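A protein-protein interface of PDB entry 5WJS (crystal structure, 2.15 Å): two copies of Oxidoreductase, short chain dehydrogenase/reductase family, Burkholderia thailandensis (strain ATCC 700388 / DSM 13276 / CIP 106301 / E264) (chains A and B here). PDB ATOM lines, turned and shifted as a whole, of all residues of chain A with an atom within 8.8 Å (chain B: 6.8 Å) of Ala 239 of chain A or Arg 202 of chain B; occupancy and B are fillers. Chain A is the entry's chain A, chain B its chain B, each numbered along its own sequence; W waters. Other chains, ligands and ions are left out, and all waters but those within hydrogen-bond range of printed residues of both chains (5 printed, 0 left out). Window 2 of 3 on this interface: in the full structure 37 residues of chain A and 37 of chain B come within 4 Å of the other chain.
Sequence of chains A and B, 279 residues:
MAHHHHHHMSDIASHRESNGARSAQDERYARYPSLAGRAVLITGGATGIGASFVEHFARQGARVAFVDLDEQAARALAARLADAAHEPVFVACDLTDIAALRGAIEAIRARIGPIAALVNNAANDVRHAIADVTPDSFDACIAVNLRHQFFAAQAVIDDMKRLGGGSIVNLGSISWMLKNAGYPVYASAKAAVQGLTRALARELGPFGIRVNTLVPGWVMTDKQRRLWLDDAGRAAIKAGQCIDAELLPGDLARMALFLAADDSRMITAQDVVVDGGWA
The backbone carbonyl oxygen (O) of Gly 240 of chain A lies within hydrogen-bond range of the guanidinium group (NH1) of Arg 202 of chain B, at 3.1 Å.
The backbone NH (N) of Arg 202 of chain B lies close to the side-chain sulfur (SG) of Cys 242 of chain A, at 3.8 Å.
NE2 of Gln 241 of chain A lies within hydrogen-bond range of O of Ile 243 of chain A (2.9 Å).
O of Gly 276 of chain A lies within hydrogen-bond range of N of Cys 242 of chain A (2.7 Å).
The side-chain sulfur (SG) of Cys 242 of chain A sits at hydrogen-bond distance from the backbone carbonyl oxygen (O) of Gly 277 of chain A (3.5 Å).
N of Ile 243 of chain A lies within hydrogen-bond range of O of Gly 276 of chain A (3.2 Å).
The backbone NH of Val 211 of chain B lies within hydrogen-bond range of the side-chain hydroxyl of Thr 268 of chain B.
Among the printed residues, merely in contact across the chains: Ala 239 of chain A with Arg 202 of chain B (3.5 Å), Gln 241 of chain A with Arg 202 of chain B (3.9 Å), Cys 242 of chain A with Ala 201 of chain B (3.5 Å), Cys 242 of chain A with Gly 205 of chain B (3.3 Å), Cys 242 of chain A with Pro 206 of chain B (3.6 Å), Ile 243 of chain A with Gly 205 of chain B (3.9 Å), Ile 243 of chain A with Thr 268 of chain B (3.7 Å), Gly 276 of chain A with Thr 268 of chain B (3.7 Å) and Gly 277 of chain A with Thr 268 of chain B (3.5 Å).
Of chain B, only Arg 202 comes within 4 Å of Ala 239 of chain A.
Ala 201 of chain B touches just one residue of chain A: Cys 242.
Of the printed residues of chain B, Ile 243 of chain A touches Gly 205 (3.9 Å) and Thr 268 (3.7 Å).
Of the printed residues of chain B, Cys 242 of chain A touches Ala 201, Arg 202, Gly 205 and Pro 206.
Printed residues of chain A within 4 Å of Thr 268 of chain B: Ile 243, Gly 276 and Gly 277.
Of the printed residues of chain A, Pro 206 of chain B touches Cys 242.
The nearest printed residue of chain B that does not touch Ala 239 of chain A is Pro 206 of chain B (9.3 Å).
The nearest printed residue of chain B that does not touch Ile 243 of chain A is Ile 209 of chain B (4.9 Å).
Hydrophobic or aromatic side chains of chain A that line the printed part of chain B: Ile 243.
Along chain A the printed residues that touch a printed residue of chain B span positions 239 to 277.
Of the 14 printed residues of chain B, 5 touch a printed residue of chain A.
Hydrophobic or aromatic side chains of chain B that line the printed part of chain A: Pro 206.
Along chain B the printed residues that touch a printed residue of chain A span positions 201 to 268.
No position is printed for both chains.
Of the 11 pairs that touch across the chains among the printed residues, none has its exchanged pair printed and touching as well.
Water W4 lies within hydrogen-bond range of O of Arg 202 of chain B and O of Cys 242 of chain A.
Water W1 lies within hydrogen-bond range of O of Gly 240 of chain A (2.7 Å), O of Trp 278 of chain A (2.8 Å) and NH2 of Arg 202 of chain B (3.0 Å).
Water W2 bridges the chain-end carboxylate of Ala 279 of chain A and the guanidinium group of Arg 198 of chain B.
Water W5 bridges O of Ala 239 of chain A (2.8 Å) and NH1 of Arg 202 of chain B (3.5 Å).
Water W3 lies within hydrogen-bond range of the guanidinium group of Arg 202 of chain B and the backbone carbonyl oxygen of Gln 241 of chain A.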
ATOM      1  N   ALA A 232      -1.531  29.214   8.950  1.00  0.00           N
ATOM      2  CA  ALA A 232      -1.440  28.281   7.832  1.00  0.00           C
ATOM      3  C   ALA A 232      -0.352  27.244   8.069  1.00  0.00           C
ATOM      4  O   ALA A 232      -0.607  26.036   7.996  1.00  0.00           O
ATOM      5  CB  ALA A 232      -1.172  29.038   6.533  1.00  0.00           C
ATOM      6  N   GLY A 233       0.872  27.702   8.350  1.00  0.00           N
ATOM      7  CA  GLY A 233       1.962  26.776   8.611  1.00  0.00           C
ATOM      8  C   GLY A 233       1.643  25.800   9.728  1.00  0.00           C
ATOM      9  O   GLY A 233       1.872  24.594   9.593  1.00  0.00           O
ATOM     10  N   ARG A 234       1.089  26.305  10.838  1.00  0.00           N
ATOM     11  CA  ARG A 234       0.755  25.435  11.961  1.00  0.00           C
ATOM     12  C   ARG A 234      -0.216  24.337  11.541  1.00  0.00           C
ATOM     13  O   ARG A 234      -0.067  23.180  11.952  1.00  0.00           O
ATOM     14  CB  ARG A 234       0.176  26.260  13.116  1.00  0.00           C
ATOM     15  CG  ARG A 234       1.234  26.847  14.054  1.00  0.00           C
ATOM     16  CD  ARG A 234       0.613  27.694  15.161  1.00  0.00           C
ATOM     17  NE  ARG A 234       0.266  29.036  14.696  1.00  0.00           N
ATOM     18  CZ  ARG A 234       1.135  30.042  14.620  1.00  0.00           C
ATOM     19  NH1 ARG A 234       0.740  31.232  14.184  1.00  0.00           N
ATOM     20  NH2 ARG A 234       2.402  29.853  14.976  1.00  0.00           N
ATOM     21  N   ALA A 235      -1.210  24.680  10.714  1.00  0.00           N
ATOM     22  CA  ALA A 235      -2.173  23.687  10.242  1.00  0.00           C
ATOM     23  C   ALA A 235      -1.509  22.637   9.353  1.00  0.00           C
ATOM     24  O   ALA A 235      -1.829  21.445   9.447  1.00  0.00           O
ATOM     25  CB  ALA A 235      -3.311  24.376   9.487  1.00  0.00           C
ATOM     26  N   ALA A 236      -0.594  23.058   8.473  1.00  0.00           N
ATOM     27  CA  ALA A 236       0.069  22.098   7.598  1.00  0.00           C
ATOM     28  C   ALA A 236       0.953  21.161   8.400  1.00  0.00           C
ATOM     29  O   ALA A 236       1.003  19.955   8.127  1.00  0.00           O
ATOM     30  CB  ALA A 236       0.883  22.824   6.529  1.00  0.00           C
ATOM     31  N   ILE A 237       1.654  21.703   9.400  1.00  0.00           N
ATOM     32  CA  ILE A 237       2.514  20.891  10.248  1.00  0.00           C
ATOM     33  C   ILE A 237       1.698  19.809  10.946  1.00  0.00           C
ATOM     34  O   ILE A 237       2.073  18.629  10.947  1.00  0.00           O
ATOM     35  CB  ILE A 237       3.259  21.783  11.254  1.00  0.00           C
ATOM     36  CG1 ILE A 237       4.273  22.664  10.518  1.00  0.00           C
ATOM     37  CG2 ILE A 237       3.913  20.942  12.342  1.00  0.00           C
ATOM     38  CD1 ILE A 237       4.939  23.736  11.387  1.00  0.00           C
ATOM     39  N   LYS A 238       0.548  20.192  11.515  1.00  0.00           N
ATOM     40  CA  LYS A 238      -0.264  19.245  12.279  1.00  0.00           C
ATOM     41  C   LYS A 238      -0.851  18.159  11.384  1.00  0.00           C
ATOM     42  O   LYS A 238      -0.841  16.974  11.741  1.00  0.00           O
ATOM     43  CB  LYS A 238      -1.378  19.983  13.030  1.00  0.00           C
ATOM     44  N   ALA A 239      -1.366  18.539  10.216  1.00  0.00           N
ATOM     45  CA  ALA A 239      -1.884  17.532   9.295  1.00  0.00           C
ATOM     46  C   ALA A 239      -0.763  16.684   8.699  1.00  0.00           C
ATOM     47  O   ALA A 239      -0.970  15.499   8.419  1.00  0.00           O
ATOM     48  CB  ALA A 239      -2.700  18.199   8.189  1.00  0.00           C
ATOM     49  N   GLY A 240       0.428  17.252   8.520  1.00  0.00           N
ATOM     50  CA  GLY A 240       1.499  16.527   7.869  1.00  0.00           C
ATOM     51  C   GLY A 240       2.265  15.587   8.782  1.00  0.00           C
ATOM     52  O   GLY A 240       2.419  14.402   8.464  1.00  0.00           O
ATOM     53  N   GLN A 241       2.775  16.104   9.899  1.00  0.00           N
ATOM     54  CA  GLN A 241       3.513  15.276  10.842  1.00  0.00           C
ATOM     55  C   GLN A 241       2.599  14.231  11.478  1.00  0.00           C
ATOM     56  O   GLN A 241       1.417  14.479  11.735  1.00  0.00           O
ATOM     57  CB  GLN A 241       4.145  16.137  11.936  1.00  0.00           C
ATOM     58  CG  GLN A 241       5.296  17.015  11.464  1.00  0.00           C
ATOM     59  CD  GLN A 241       5.818  17.936  12.557  1.00  0.00           C
ATOM     60  OE1 GLN A 241       6.689  18.778  12.309  1.00  0.00           O
ATOM     61  NE2 GLN A 241       5.292  17.778  13.776  1.00  0.00           N
ATOM     62  N   CYS A 242       3.160  13.042  11.715  1.00  0.00           N
ATOM     63  CA  CYS A 242       2.462  12.038  12.511  1.00  0.00           C
ATOM     64  C   CYS A 242       2.373  12.444  13.977  1.00  0.00           C
ATOM     65  O   CYS A 242       1.398  12.103  14.659  1.00  0.00           O
ATOM     66  CB  CYS A 242       3.162  10.681  12.393  1.00  0.00           C
ATOM     67  SG  CYS A 242       3.011   9.868  10.772  1.00  0.00           S
ATOM     68  N   ILE A 243       3.381  13.139  14.487  1.00  0.00           N
ATOM     69  CA  ILE A 243       3.415  13.564  15.881  1.00  0.00           C
ATOM     70  C   ILE A 243       3.088  15.048  15.932  1.00  0.00           C
ATOM     71  O   ILE A 243       3.773  15.868  15.305  1.00  0.00           O
ATOM     72  CB  ILE A 243       4.783  13.282  16.523  1.00  0.00           C
ATOM     73  CG1 ILE A 243       5.085  11.781  16.500  1.00  0.00           C
ATOM     74  CG2 ILE A 243       4.822  13.830  17.966  1.00  0.00           C
ATOM     75  CD1 ILE A 243       6.483  11.444  16.956  1.00  0.00           C
ATOM     76  N   ASP A 244       2.058  15.392  16.696  1.00  0.00           N
ATOM     77  CA  ASP A 244       1.568  16.767  16.807  1.00  0.00           C
ATOM     78  C   ASP A 244       2.366  17.503  17.887  1.00  0.00           C
ATOM     79  O   ASP A 244       1.875  17.821  18.971  1.00  0.00           O
ATOM     80  CB  ASP A 244       0.072  16.764  17.107  1.00  0.00           C
ATOM     81  CG  ASP A 244      -0.503  18.164  17.299  1.00  0.00           C
ATOM     82  OD1 ASP A 244       0.093  19.147  16.804  1.00  0.00           O
ATOM     83  OD2 ASP A 244      -1.561  18.274  17.958  1.00  0.00           O
ATOM     84  N   GLY A 276       9.183  14.153  12.364  1.00  0.00           N
ATOM     85  CA  GLY A 276       7.877  13.890  12.940  1.00  0.00           C
ATOM     86  C   GLY A 276       6.947  13.069  12.071  1.00  0.00           C
ATOM     87  O   GLY A 276       5.745  13.044  12.329  1.00  0.00           O
ATOM     88  N   GLY A 277       7.463  12.417  11.030  1.00  0.00           N
ATOM     89  CA  GLY A 277       6.654  11.543  10.205  1.00  0.00           C
ATOM     90  C   GLY A 277       5.972  12.211   9.032  1.00  0.00           C
ATOM     91  O   GLY A 277       5.019  11.642   8.483  1.00  0.00           O
ATOM     92  N   TRP A 278       6.426  13.401   8.629  1.00  0.00           N
ATOM     93  CA  TRP A 278       5.744  14.161   7.584  1.00  0.00           C
ATOM     94  C   TRP A 278       6.041  13.585   6.196  1.00  0.00           C
ATOM     95  O   TRP A 278       5.135  13.125   5.495  1.00  0.00           O
ATOM     96  CB  TRP A 278       6.159  15.648   7.665  1.00  0.00           C
ATOM     97  CG  TRP A 278       5.313  16.594   6.833  1.00  0.00           C
ATOM     98  CD1 TRP A 278       4.492  16.267   5.779  1.00  0.00           C
ATOM     99  CD2 TRP A 278       5.182  18.019   7.008  1.00  0.00           C
ATOM    100  NE1 TRP A 278       3.866  17.395   5.294  1.00  0.00           N
ATOM    101  CE2 TRP A 278       4.267  18.481   6.031  1.00  0.00           C
ATOM    102  CE3 TRP A 278       5.751  18.949   7.892  1.00  0.00           C
ATOM    103  CZ2 TRP A 278       3.912  19.838   5.910  1.00  0.00           C
ATOM    104  CZ3 TRP A 278       5.393  20.293   7.777  1.00  0.00           C
ATOM    105  CH2 TRP A 278       4.482  20.722   6.790  1.00  0.00           C
ATOM    106  N   ALA A 279       7.302  13.623   5.777  1.00  0.00           N
ATOM    107  CA  ALA A 279       7.659  13.318   4.395  1.00  0.00           C
ATOM    108  C   ALA A 279       7.489  11.845   4.050  1.00  0.00           C
ATOM    109  O   ALA A 279       7.488  11.534   2.853  1.00  0.00           O
ATOM    110  CB  ALA A 279       9.084  13.740   4.103  1.00  0.00           C
ATOM    111  OXT ALA A 279       7.376  10.979   4.930  1.00  0.00           O
ATOM    112  N   THR B 197       4.426  -0.129   9.603  1.00  0.00           N
ATOM    113  CA  THR B 197       5.065   0.957  10.336  1.00  0.00           C
ATOM    114  C   THR B 197       4.390   2.291  10.033  1.00  0.00           C
ATOM    115  O   THR B 197       4.056   3.057  10.948  1.00  0.00           O
ATOM    116  CB  THR B 197       6.556   0.990   9.982  1.00  0.00           C
ATOM    117  OG1 THR B 197       7.225  -0.057  10.702  1.00  0.00           O
ATOM    118  CG2 THR B 197       7.195   2.337  10.332  1.00  0.00           C
ATOM    119  N   ARG B 198       4.149   2.570   8.751  1.00  0.00           N
ATOM    120  CA  ARG B 198       3.618   3.876   8.384  1.00  0.00           C
ATOM    121  C   ARG B 198       2.165   4.019   8.847  1.00  0.00           C
ATOM    122  O   ARG B 198       1.775   5.075   9.352  1.00  0.00           O
ATOM    123  CB  ARG B 198       3.783   4.095   6.871  1.00  0.00           C
ATOM    124  CG  ARG B 198       5.276   4.116   6.441  1.00  0.00           C
ATOM    125  CD  ARG B 198       5.493   3.896   4.938  1.00  0.00           C
ATOM    126  NE  ARG B 198       5.216   5.114   4.182  1.00  0.00           N
ATOM    127  CZ  ARG B 198       6.070   6.120   4.038  1.00  0.00           C
ATOM    128  NH1 ARG B 198       7.278   6.041   4.591  1.00  0.00           N
ATOM    129  NH2 ARG B 198       5.714   7.202   3.346  1.00  0.00           N
ATOM    130  N   ALA B 199       1.359   2.954   8.740  1.00  0.00           N
ATOM    131  CA  ALA B 199      -0.023   3.053   9.209  1.00  0.00           C
ATOM    132  C   ALA B 199      -0.079   3.214  10.727  1.00  0.00           C
ATOM    133  O   ALA B 199      -0.836   4.046  11.230  1.00  0.00           O
ATOM    134  CB  ALA B 199      -0.841   1.850   8.760  1.00  0.00           C
ATOM    135  N   LEU B 200       0.721   2.447  11.474  1.00  0.00           N
ATOM    136  CA  LEU B 200       0.730   2.608  12.926  1.00  0.00           C
ATOM    137  C   LEU B 200       1.254   3.983  13.327  1.00  0.00           C
ATOM    138  O   LEU B 200       0.750   4.600  14.275  1.00  0.00           O
ATOM    139  CB  LEU B 200       1.575   1.521  13.587  1.00  0.00           C
ATOM    140  CG  LEU B 200       1.089   0.090  13.378  1.00  0.00           C
ATOM    141  CD1 LEU B 200       1.895  -0.856  14.240  1.00  0.00           C
ATOM    142  CD2 LEU B 200      -0.377  -0.004  13.692  1.00  0.00           C
ATOM    143  N   ALA B 201       2.278   4.468  12.625  1.00  0.00           N
ATOM    144  CA  ALA B 201       2.879   5.748  12.979  1.00  0.00           C
ATOM    145  C   ALA B 201       1.864   6.874  12.864  1.00  0.00           C
ATOM    146  O   ALA B 201       1.822   7.770  13.714  1.00  0.00           O
ATOM    147  CB  ALA B 201       4.102   6.023  12.091  1.00  0.00           C
ATOM    148  N   ARG B 202       1.028   6.841  11.825  1.00  0.00           N
ATOM    149  CA  ARG B 202      -0.013   7.856  11.685  1.00  0.00           C
ATOM    150  C   ARG B 202      -1.012   7.779  12.833  1.00  0.00           C
ATOM    151  O   ARG B 202      -1.354   8.795  13.448  1.00  0.00           O
ATOM    152  CB  ARG B 202      -0.736   7.697  10.350  1.00  0.00           C
ATOM    153  CG  ARG B 202      -1.897   8.699  10.165  1.00  0.00           C
ATOM    154  CD  ARG B 202      -1.325  10.080   9.817  1.00  0.00           C
ATOM    155  NE  ARG B 202      -0.620  10.084   8.533  1.00  0.00           N
ATOM    156  CZ  ARG B 202       0.110  11.098   8.062  1.00  0.00           C
ATOM    157  NH1 ARG B 202       0.257  12.211   8.777  1.00  0.00           N
ATOM    158  NH2 ARG B 202       0.701  11.001   6.866  1.00  0.00           N
ATOM    159  N   GLU B 203      -1.501   6.577  13.131  1.00  0.00           N
ATOM    160  CA  GLU B 203      -2.541   6.447  14.146  1.00  0.00           C
ATOM    161  C   GLU B 203      -2.010   6.671  15.552  1.00  0.00           C
ATOM    162  O   GLU B 203      -2.755   7.115  16.426  1.00  0.00           O
ATOM    163  CB  GLU B 203      -3.189   5.067  14.081  1.00  0.00           C
ATOM    164  CG  GLU B 203      -4.214   4.912  13.000  1.00  0.00           C
ATOM    165  CD  GLU B 203      -5.139   3.764  13.283  1.00  0.00           C
ATOM    166  OE1 GLU B 203      -5.520   3.599  14.461  1.00  0.00           O
ATOM    167  OE2 GLU B 203      -5.469   3.024  12.334  1.00  0.00           O
ATOM    168  N   LEU B 204      -0.751   6.341  15.814  1.00  0.00           N
ATOM    169  CA  LEU B 204      -0.304   6.331  17.201  1.00  0.00           C
ATOM    170  C   LEU B 204       0.498   7.567  17.572  1.00  0.00           C
ATOM    171  O   LEU B 204       0.645   7.861  18.767  1.00  0.00           O
ATOM    172  CB  LEU B 204       0.507   5.063  17.477  1.00  0.00           C
ATOM    173  CG  LEU B 204      -0.250   3.742  17.288  1.00  0.00           C
ATOM    174  CD1 LEU B 204       0.709   2.542  17.378  1.00  0.00           C
ATOM    175  CD2 LEU B 204      -1.410   3.594  18.292  1.00  0.00           C
ATOM    176  N   GLY B 205       0.986   8.310  16.571  1.00  0.00           N
ATOM    177  CA  GLY B 205       1.681   9.554  16.792  1.00  0.00           C
ATOM    178  C   GLY B 205       0.939  10.582  17.621  1.00  0.00           C
ATOM    179  O   GLY B 205       1.566  11.264  18.439  1.00  0.00           O
ATOM    180  N   PRO B 206      -0.383  10.730  17.455  1.00  0.00           N
ATOM    181  CA  PRO B 206      -1.120  11.619  18.374  1.00  0.00           C
ATOM    182  C   PRO B 206      -0.951  11.260  19.844  1.00  0.00           C
ATOM    183  O   PRO B 206      -1.253  12.099  20.703  1.00  0.00           O
ATOM    184  CB  PRO B 206      -2.580  11.462  17.921  1.00  0.00           C
ATOM    185  CG  PRO B 206      -2.473  11.166  16.458  1.00  0.00           C
ATOM    186  CD  PRO B 206      -1.245  10.277  16.345  1.00  0.00           C
ATOM    187  N   ILE B 209       3.563   8.038  20.414  1.00  0.00           N
ATOM    188  CA  ILE B 209       4.129   6.735  20.089  1.00  0.00           C
ATOM    189  C   ILE B 209       4.788   6.836  18.719  1.00  0.00           C
ATOM    190  O   ILE B 209       4.115   7.115  17.720  1.00  0.00           O
ATOM    191  CB  ILE B 209       3.047   5.644  20.109  1.00  0.00           C
ATOM    192  CG1 ILE B 209       2.476   5.491  21.522  1.00  0.00           C
ATOM    193  CG2 ILE B 209       3.592   4.325  19.551  1.00  0.00           C
ATOM    194  CD1 ILE B 209       1.137   4.769  21.559  1.00  0.00           C
ATOM    195  N   VAL B 211       6.705   4.892  15.646  1.00  0.00           N
ATOM    196  CA  VAL B 211       6.827   3.576  15.034  1.00  0.00           C
ATOM    197  C   VAL B 211       7.813   3.684  13.880  1.00  0.00           C
ATOM    198  O   VAL B 211       7.631   4.514  12.984  1.00  0.00           O
ATOM    199  CB  VAL B 211       5.475   3.037  14.537  1.00  0.00           C
ATOM    200  CG1 VAL B 211       5.619   1.560  14.122  1.00  0.00           C
ATOM    201  CG2 VAL B 211       4.389   3.227  15.607  1.00  0.00           C
ATOM    202  N   THR B 268       9.811   9.139  13.476  1.00  0.00           N
ATOM    203  CA  THR B 268       8.776   8.127  13.359  1.00  0.00           C
ATOM    204  C   THR B 268       8.448   7.954  11.884  1.00  0.00           C
ATOM    205  O   THR B 268       8.759   8.820  11.060  1.00  0.00           O
ATOM    206  CB  THR B 268       7.538   8.483  14.196  1.00  0.00           C
ATOM    207  OG1 THR B 268       6.600   7.404  14.144  1.00  0.00           O
ATOM    208  CG2 THR B 268       6.871   9.788  13.705  1.00  0.00           C
ATOM    209  N   ALA B 269       7.855   6.795  11.563  1.00  0.00           N
ATOM    210  CA  ALA B 269       7.481   6.375  10.210  1.00  0.00           C
ATOM    211  C   ALA B 269       8.686   6.192   9.284  1.00  0.00           C
ATOM    212  O   ALA B 269       8.536   6.264   8.063  1.00  0.00           O
ATOM    213  CB  ALA B 269       6.484   7.346   9.573  1.00  0.00           C
HETATM  214  O   HOH W   1       2.425  13.269   5.990  1.00  0.00           O
HETATM  215  O   HOH W   2       7.596   8.942   1.947  1.00  0.00           O
HETATM  216  O   HOH W   3      -1.219  13.248  11.116  1.00  0.00           O
HETATM  217  O   HOH W   4      -1.190  11.469  13.042  1.00  0.00           O
HETATM  218  O   HOH W   5      -2.945  13.530   8.780  1.00  0.00           O
